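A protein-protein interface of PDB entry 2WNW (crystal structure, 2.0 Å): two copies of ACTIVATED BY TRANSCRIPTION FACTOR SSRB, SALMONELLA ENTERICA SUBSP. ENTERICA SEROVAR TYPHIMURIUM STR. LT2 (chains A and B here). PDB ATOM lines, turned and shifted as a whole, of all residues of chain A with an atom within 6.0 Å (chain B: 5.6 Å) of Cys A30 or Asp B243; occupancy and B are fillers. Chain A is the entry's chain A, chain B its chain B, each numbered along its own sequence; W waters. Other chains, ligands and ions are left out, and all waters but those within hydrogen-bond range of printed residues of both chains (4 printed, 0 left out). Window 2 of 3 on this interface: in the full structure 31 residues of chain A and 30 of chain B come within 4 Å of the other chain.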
ATOM      1  N   ARG A  26     -40.227  -8.108  -8.447  1.00  0.00           N
ATOM      2  CA  ARG A  26     -39.065  -8.185  -7.567  1.00  0.00           C
ATOM      3  C   ARG A  26     -39.176  -7.346  -6.299  1.00  0.00           C
ATOM      4  O   ARG A  26     -39.861  -6.323  -6.265  1.00  0.00           O
ATOM      5  CB  ARG A  26     -37.790  -7.779  -8.310  1.00  0.00           C
ATOM      6  CG  ARG A  26     -37.638  -6.282  -8.540  1.00  0.00           C
ATOM      7  CD  ARG A  26     -36.165  -5.909  -8.692  1.00  0.00           C
ATOM      8  NE  ARG A  26     -35.417  -6.182  -7.467  1.00  0.00           N
ATOM      9  CZ  ARG A  26     -34.093  -6.134  -7.363  1.00  0.00           C
ATOM     10  NH1 ARG A  26     -33.348  -5.818  -8.414  1.00  0.00           N
ATOM     11  NH2 ARG A  26     -33.509  -6.411  -6.204  1.00  0.00           N
ATOM     12  N   GLN A  27     -38.494  -7.802  -5.254  1.00  0.00           N
ATOM     13  CA  GLN A  27     -38.463  -7.100  -3.981  1.00  0.00           C
ATOM     14  C   GLN A  27     -37.276  -6.149  -4.080  1.00  0.00           C
ATOM     15  O   GLN A  27     -36.346  -6.396  -4.849  1.00  0.00           O
ATOM     16  CB  GLN A  27     -38.230  -8.080  -2.835  1.00  0.00           C
ATOM     17  CG  GLN A  27     -39.172  -9.267  -2.824  1.00  0.00           C
ATOM     18  CD  GLN A  27     -38.792 -10.289  -1.770  1.00  0.00           C
ATOM     19  OE1 GLN A  27     -38.832 -10.005  -0.574  1.00  0.00           O
ATOM     20  NE2 GLN A  27     -38.413 -11.483  -2.210  1.00  0.00           N
ATOM     21  N   ARG A  28     -37.306  -5.070  -3.305  1.00  0.00           N
ATOM     22  CA  ARG A  28     -36.223  -4.095  -3.326  1.00  0.00           C
ATOM     23  C   ARG A  28     -34.881  -4.682  -2.893  1.00  0.00           C
ATOM     24  O   ARG A  28     -33.844  -4.349  -3.464  1.00  0.00           O
ATOM     25  CB  ARG A  28     -36.574  -2.891  -2.443  1.00  0.00           C
ATOM     26  CG  ARG A  28     -37.401  -1.819  -3.150  1.00  0.00           C
ATOM     27  CD  ARG A  28     -37.605  -0.594  -2.261  1.00  0.00           C
ATOM     28  NE  ARG A  28     -38.831  -0.669  -1.470  1.00  0.00           N
ATOM     29  CZ  ARG A  28     -40.043  -0.384  -1.941  1.00  0.00           C
ATOM     30  NH1 ARG A  28     -40.194  -0.002  -3.204  1.00  0.00           N
ATOM     31  NH2 ARG A  28     -41.106  -0.481  -1.151  1.00  0.00           N
ATOM     32  N   ASP A  29     -34.901  -5.550  -1.884  1.00  0.00           N
ATOM     33  CA  ASP A  29     -33.674  -6.171  -1.387  1.00  0.00           C
ATOM     34  C   ASP A  29     -32.903  -6.827  -2.526  1.00  0.00           C
ATOM     35  O   ASP A  29     -33.502  -7.416  -3.426  1.00  0.00           O
ATOM     36  CB  ASP A  29     -33.995  -7.228  -0.330  1.00  0.00           C
ATOM     37  CG  ASP A  29     -32.773  -8.040   0.066  1.00  0.00           C
ATOM     38  OD1 ASP A  29     -31.902  -7.501   0.771  1.00  0.00           O
ATOM     39  OD2 ASP A  29     -32.679  -9.214  -0.339  1.00  0.00           O
ATOM     40  N   CYS A  30     -31.576  -6.736  -2.476  1.00  0.00           N
ATOM     41  CA  CYS A  30     -30.729  -7.317  -3.517  1.00  0.00           C
ATOM     42  C   CYS A  30     -29.841  -8.466  -3.046  1.00  0.00           C
ATOM     43  O   CYS A  30     -28.837  -8.776  -3.686  1.00  0.00           O
ATOM     44  CB  CYS A  30     -29.842  -6.234  -4.139  1.00  0.00           C
ATOM     45  SG  CYS A  30     -30.745  -4.980  -5.079  1.00  0.00           S
ATOM     46  N   SER A  31     -30.206  -9.108  -1.941  1.00  0.00           N
ATOM     47  CA  SER A  31     -29.402 -10.211  -1.427  1.00  0.00           C
ATOM     48  C   SER A  31     -29.838 -11.564  -1.989  1.00  0.00           C
ATOM     49  O   SER A  31     -30.968 -11.715  -2.465  1.00  0.00           O
ATOM     50  CB  SER A  31     -29.481 -10.252   0.100  1.00  0.00           C
ATOM     51  OG  SER A  31     -30.774 -10.640   0.524  1.00  0.00           O
ATOM     52  N   GLU A  32     -28.928 -12.535  -1.927  1.00  0.00           N
ATOM     53  CA  GLU A  32     -29.170 -13.901  -2.395  1.00  0.00           C
ATOM     54  C   GLU A  32     -29.670 -14.002  -3.825  1.00  0.00           C
ATOM     55  O   GLU A  32     -30.497 -14.859  -4.148  1.00  0.00           O
ATOM     56  CB  GLU A  32     -30.155 -14.612  -1.460  1.00  0.00           C
ATOM     57  CG  GLU A  32     -29.586 -14.883  -0.080  1.00  0.00           C
ATOM     58  CD  GLU A  32     -30.548 -15.635   0.824  1.00  0.00           C
ATOM     59  OE1 GLU A  32     -30.121 -16.037   1.923  1.00  0.00           O
ATOM     60  OE2 GLU A  32     -31.724 -15.821   0.445  1.00  0.00           O
ATOM     61  N   LEU A  33     -29.137 -13.153  -4.692  1.00  0.00           N
ATOM     62  CA  LEU A  33     -29.556 -13.134  -6.082  1.00  0.00           C
ATOM     63  C   LEU A  33     -28.735 -13.935  -7.074  1.00  0.00           C
ATOM     64  O   LEU A  33     -27.528 -14.089  -6.931  1.00  0.00           O
ATOM     65  CB  LEU A  33     -29.564 -11.699  -6.608  1.00  0.00           C
ATOM     66  CG  LEU A  33     -30.461 -10.632  -5.985  1.00  0.00           C
ATOM     67  CD1 LEU A  33     -30.211  -9.310  -6.702  1.00  0.00           C
ATOM     68  CD2 LEU A  33     -31.920 -11.045  -6.116  1.00  0.00           C
ATOM     69  N   SER A  35     -28.659 -13.244 -10.754  1.00  0.00           N
ATOM     70  CA  SER A  35     -29.146 -12.309 -11.755  1.00  0.00           C
ATOM     71  C   SER A  35     -28.989 -12.855 -13.161  1.00  0.00           C
ATOM     72  O   SER A  35     -27.940 -13.394 -13.511  1.00  0.00           O
ATOM     73  CB  SER A  35     -28.388 -10.986 -11.643  1.00  0.00           C
ATOM     74  OG  SER A  35     -28.469 -10.464 -10.329  1.00  0.00           O
ATOM     75  N   SER A 387     -25.173 -13.971 -13.180  1.00  0.00           N
ATOM     76  CA  SER A 387     -24.221 -13.931 -12.076  1.00  0.00           C
ATOM     77  C   SER A 387     -24.867 -14.445 -10.798  1.00  0.00           C
ATOM     78  O   SER A 387     -26.077 -14.300 -10.592  1.00  0.00           O
ATOM     79  CB  SER A 387     -23.683 -12.507 -11.862  1.00  0.00           C
ATOM     80  OG  SER A 387     -24.690 -11.609 -11.424  1.00  0.00           O
ATOM     81  N   ARG A 420     -32.660 -16.156  -5.354  1.00  0.00           N
ATOM     82  CA  ARG A 420     -33.765 -15.524  -6.039  1.00  0.00           C
ATOM     83  C   ARG A 420     -33.318 -15.274  -7.464  1.00  0.00           C
ATOM     84  O   ARG A 420     -32.403 -14.483  -7.699  1.00  0.00           O
ATOM     85  CB  ARG A 420     -34.133 -14.194  -5.378  1.00  0.00           C
ATOM     86  CG  ARG A 420     -34.877 -14.318  -4.061  1.00  0.00           C
ATOM     87  CD  ARG A 420     -35.408 -12.953  -3.639  1.00  0.00           C
ATOM     88  NE  ARG A 420     -34.338 -12.060  -3.223  1.00  0.00           N
ATOM     89  CZ  ARG A 420     -34.333 -10.744  -3.417  1.00  0.00           C
ATOM     90  NH1 ARG A 420     -35.344 -10.150  -4.037  1.00  0.00           N
ATOM     91  NH2 ARG A 420     -33.317 -10.019  -2.974  1.00  0.00           N
ATOM     92  N   TRP B 238     -21.517   4.623 -10.070  1.00  0.00           N
ATOM     93  CA  TRP B 238     -22.133   3.444  -9.454  1.00  0.00           C
ATOM     94  C   TRP B 238     -21.768   3.423  -7.969  1.00  0.00           C
ATOM     95  O   TRP B 238     -22.576   3.804  -7.129  1.00  0.00           O
ATOM     96  CB  TRP B 238     -21.677   2.141 -10.123  1.00  0.00           C
ATOM     97  CG  TRP B 238     -22.359   0.904  -9.562  1.00  0.00           C
ATOM     98  CD1 TRP B 238     -21.751  -0.254  -9.163  1.00  0.00           C
ATOM     99  CD2 TRP B 238     -23.772   0.699  -9.375  1.00  0.00           C
ATOM    100  NE1 TRP B 238     -22.693  -1.167  -8.741  1.00  0.00           N
ATOM    101  CE2 TRP B 238     -23.940  -0.609  -8.862  1.00  0.00           C
ATOM    102  CE3 TRP B 238     -24.911   1.492  -9.593  1.00  0.00           C
ATOM    103  CZ2 TRP B 238     -25.200  -1.144  -8.564  1.00  0.00           C
ATOM    104  CZ3 TRP B 238     -26.167   0.960  -9.297  1.00  0.00           C
ATOM    105  CH2 TRP B 238     -26.299  -0.347  -8.787  1.00  0.00           C
ATOM    106  N   ASP B 241     -23.151  -2.124  -4.975  1.00  0.00           N
ATOM    107  CA  ASP B 241     -22.929  -3.567  -5.075  1.00  0.00           C
ATOM    108  C   ASP B 241     -22.832  -4.123  -6.489  1.00  0.00           C
ATOM    109  O   ASP B 241     -23.330  -3.531  -7.440  1.00  0.00           O
ATOM    110  CB  ASP B 241     -23.993  -4.294  -4.261  1.00  0.00           C
ATOM    111  CG  ASP B 241     -24.096  -3.749  -2.857  1.00  0.00           C
ATOM    112  OD1 ASP B 241     -23.038  -3.614  -2.204  1.00  0.00           O
ATOM    113  OD2 ASP B 241     -25.220  -3.442  -2.410  1.00  0.00           O
ATOM    114  N   LYS B 242     -22.180  -5.276  -6.614  1.00  0.00           N
ATOM    115  CA  LYS B 242     -21.960  -5.892  -7.920  1.00  0.00           C
ATOM    116  C   LYS B 242     -23.174  -6.446  -8.668  1.00  0.00           C
ATOM    117  O   LYS B 242     -23.111  -6.640  -9.880  1.00  0.00           O
ATOM    118  CB  LYS B 242     -20.876  -6.976  -7.787  1.00  0.00           C
ATOM    119  CG  LYS B 242     -19.504  -6.409  -7.411  1.00  0.00           C
ATOM    120  CD  LYS B 242     -18.430  -7.489  -7.247  1.00  0.00           C
ATOM    121  CE  LYS B 242     -18.476  -8.142  -5.867  1.00  0.00           C
ATOM    122  NZ  LYS B 242     -17.473  -9.248  -5.753  1.00  0.00           N
ATOM    123  N   ASP B 243     -24.281  -6.685  -7.971  1.00  0.00           N
ATOM    124  CA  ASP B 243     -25.469  -7.231  -8.629  1.00  0.00           C
ATOM    125  C   ASP B 243     -26.104  -6.298  -9.668  1.00  0.00           C
ATOM    126  O   ASP B 243     -26.771  -6.761 -10.593  1.00  0.00           O
ATOM    127  CB  ASP B 243     -26.514  -7.620  -7.580  1.00  0.00           C
ATOM    128  CG  ASP B 243     -27.048  -6.422  -6.827  1.00  0.00           C
ATOM    129  OD1 ASP B 243     -28.098  -5.877  -7.234  1.00  0.00           O
ATOM    130  OD2 ASP B 243     -26.407  -6.016  -5.837  1.00  0.00           O
ATOM    131  N   GLY B 244     -25.895  -4.993  -9.530  1.00  0.00           N
ATOM    132  CA  GLY B 244     -26.481  -4.061 -10.484  1.00  0.00           C
ATOM    133  C   GLY B 244     -25.460  -3.377 -11.376  1.00  0.00           C
ATOM    134  O   GLY B 244     -25.754  -2.369 -12.018  1.00  0.00           O
ATOM    135  N   LEU B 245     -24.262  -3.950 -11.431  1.00  0.00           N
ATOM    136  CA  LEU B 245     -23.154  -3.393 -12.202  1.00  0.00           C
ATOM    137  C   LEU B 245     -23.375  -3.253 -13.710  1.00  0.00           C
ATOM    138  O   LEU B 245     -23.245  -2.154 -14.262  1.00  0.00           O
ATOM    139  CB  LEU B 245     -21.905  -4.233 -11.929  1.00  0.00           C
ATOM    140  CG  LEU B 245     -20.501  -3.708 -12.214  1.00  0.00           C
ATOM    141  CD1 LEU B 245     -20.305  -2.304 -11.657  1.00  0.00           C
ATOM    142  CD2 LEU B 245     -19.510  -4.676 -11.576  1.00  0.00           C
ATOM    143  N   VAL B 246     -23.694  -4.353 -14.382  1.00  0.00           N
ATOM    144  CA  VAL B 246     -23.906  -4.306 -15.822  1.00  0.00           C
ATOM    145  C   VAL B 246     -25.068  -3.398 -16.217  1.00  0.00           C
ATOM    146  O   VAL B 246     -24.933  -2.587 -17.130  1.00  0.00           O
ATOM    147  CB  VAL B 246     -24.138  -5.720 -16.401  1.00  0.00           C
ATOM    148  CG1 VAL B 246     -24.503  -5.632 -17.880  1.00  0.00           C
ATOM    149  CG2 VAL B 246     -22.872  -6.557 -16.229  1.00  0.00           C
ATOM    150  N   ASP B 247     -26.199  -3.529 -15.529  1.00  0.00           N
ATOM    151  CA  ASP B 247     -27.375  -2.710 -15.832  1.00  0.00           C
ATOM    152  C   ASP B 247     -27.050  -1.212 -15.833  1.00  0.00           C
ATOM    153  O   ASP B 247     -27.415  -0.482 -16.762  1.00  0.00           O
ATOM    154  CB  ASP B 247     -28.498  -2.979 -14.815  1.00  0.00           C
ATOM    155  CG  ASP B 247     -29.091  -4.381 -14.937  1.00  0.00           C
ATOM    156  OD1 ASP B 247     -29.295  -4.852 -16.077  1.00  0.00           O
ATOM    157  OD2 ASP B 247     -29.374  -5.004 -13.889  1.00  0.00           O
ATOM    158  N   THR B 271     -23.670  -7.614  -1.608  1.00  0.00           N
ATOM    159  CA  THR B 271     -24.709  -8.535  -2.066  1.00  0.00           C
ATOM    160  C   THR B 271     -24.115  -9.840  -2.608  1.00  0.00           C
ATOM    161  O   THR B 271     -24.803 -10.627  -3.264  1.00  0.00           O
ATOM    162  CB  THR B 271     -25.602  -7.912  -3.159  1.00  0.00           C
ATOM    163  OG1 THR B 271     -24.797  -7.515  -4.270  1.00  0.00           O
ATOM    164  CG2 THR B 271     -26.356  -6.701  -2.608  1.00  0.00           C
ATOM    165  N   HIS B 274     -21.093 -12.284  -7.581  1.00  0.00           N
ATOM    166  CA  HIS B 274     -21.482 -11.701  -8.865  1.00  0.00           C
ATOM    167  C   HIS B 274     -20.260 -11.368  -9.722  1.00  0.00           C
ATOM    168  O   HIS B 274     -20.242 -10.362 -10.426  1.00  0.00           O
ATOM    169  CB  HIS B 274     -22.331 -10.438  -8.634  1.00  0.00           C
ATOM    170  CG  HIS B 274     -23.678 -10.722  -8.047  1.00  0.00           C
ATOM    171  ND1 HIS B 274     -24.660 -11.404  -8.734  1.00  0.00           N
ATOM    172  CD2 HIS B 274     -24.191 -10.463  -6.819  1.00  0.00           C
ATOM    173  CE1 HIS B 274     -25.717 -11.557  -7.956  1.00  0.00           C
ATOM    174  NE2 HIS B 274     -25.458 -10.996  -6.788  1.00  0.00           N
ATOM    175  N   GLN B 277     -20.440 -10.311 -13.631  1.00  0.00           N
ATOM    176  CA  GLN B 277     -20.754  -8.970 -14.101  1.00  0.00           C
ATOM    177  C   GLN B 277     -19.491  -8.136 -14.278  1.00  0.00           C
ATOM    178  O   GLN B 277     -19.418  -7.299 -15.180  1.00  0.00           O
ATOM    179  CB  GLN B 277     -21.758  -8.291 -13.165  1.00  0.00           C
ATOM    180  CG  GLN B 277     -23.136  -8.953 -13.246  1.00  0.00           C
ATOM    181  CD  GLN B 277     -24.254  -8.093 -12.692  1.00  0.00           C
ATOM    182  OE1 GLN B 277     -24.318  -6.894 -12.961  1.00  0.00           O
ATOM    183  NE2 GLN B 277     -25.155  -8.708 -11.930  1.00  0.00           N
HETATM  184  O   HOH W   1     -26.612 -11.812  -0.669  1.00  0.00           O
HETATM  185  O   HOH W   2     -27.202 -10.931  -4.403  1.00  0.00           O
HETATM  186  O   HOH W   3     -29.322  -7.923 -10.585  1.00  0.00           O
HETATM  187  O   HOH W   4     -30.356  -6.207  -8.575  1.00  0.00           O
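No position is printed for both chains.
Cys A30 touches just these residues of chain B: Asp B243 (3.5 Å) and Thr B271 (3.4 Å).
Asp B243 touches just one residue of chain A: Cys A30.
Printed residues of chain A within 4 Å of Thr B271: Cys A30 (3.4 Å).
Of the printed residues of chain B, Leu A33 touches His B274.
Printed residues of chain B within 4 Å of Ser A387: His B274 and Gln B277.
Ser A31 touches none of the printed residues of chain B.
The nearest printed residue of chain A that does not touch Asp B243 is Leu A33 (4.1 Å).
The nearest printed residue of chain A that does not touch His B274 is Cys A30 (5.1 Å).
Among the printed residues, pairs that only touch across the chains: Cys A30 with Thr B271 (3.4 Å), Leu A33 with His B274 (3.3 Å), Ser A35 with His B274 (3.8 Å) and Ser A35 with Gln B277 (3.97 Å).
Water W4 lies within hydrogen-bond range of OD1 of Asp B243 (2.6 Å), NH1 of Arg A26 (3.0 Å) and SG of Cys A30 (3.7 Å).
Water W2 lies within hydrogen-bond range of the backbone carbonyl oxygen (O) of Thr B271 (2.7 Å), the backbone carbonyl oxygen (O) of Cys A30 (2.8 Å), a ring nitrogen (NE2) of His B274 (3.0 Å), the backbone NH (N) of Leu A33 (3.0 Å) and the backbone NH (N) of Glu A32 (3.4 Å).
Water W3 lies within hydrogen-bond range of OG of Ser A35 and O of Asp B243.
Water W1 bridges N of Glu A32 (2.7 Å) and O of Thr B271 (3.4 Å).
The side-chain sulfur (SG) of Cys A30 lies within hydrogen-bond range of the side-chain carboxylate (OD1) of Asp B243 (3.5 Å).
The side-chain hydroxyl of Ser A387 lies within hydrogen-bond range of a ring nitrogen (ND1) of His B274.
NE2 of Gln B277 sits at hydrogen-bond distance from OG of Ser A387 (3.0 Å).
NH2 of Arg A26 lies within hydrogen-bond range of SG of Cys A30 (3.3 Å).
The backbone carbonyl oxygen (O) of Arg A28 sits at hydrogen-bond distance from the side-chain sulfur (SG) of Cys A30 (3.6 Å).
The backbone NH (N) of Ser A35 is in hydrogen-bond range of the backbone carbonyl oxygen (O) of Ser A387.
The backbone carbonyl oxygen (O) of Lys B242 sits close to the side-chain amide oxygen (OE1) of Gln B277, 3.3 Å away.
The side-chain carboxylate (OD2) of Asp B243 is in hydrogen-bond range of the side-chain hydroxyl (OG1) of Thr B271 (2.7 Å).
N of Val B246 lies within hydrogen-bond range of OE1 of Gln B277 (3.0 Å).
Among the printed residues, no Asp or Glu carboxylate lies within 4 Å of a Lys or Arg side-chain nitrogen of the other chain.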
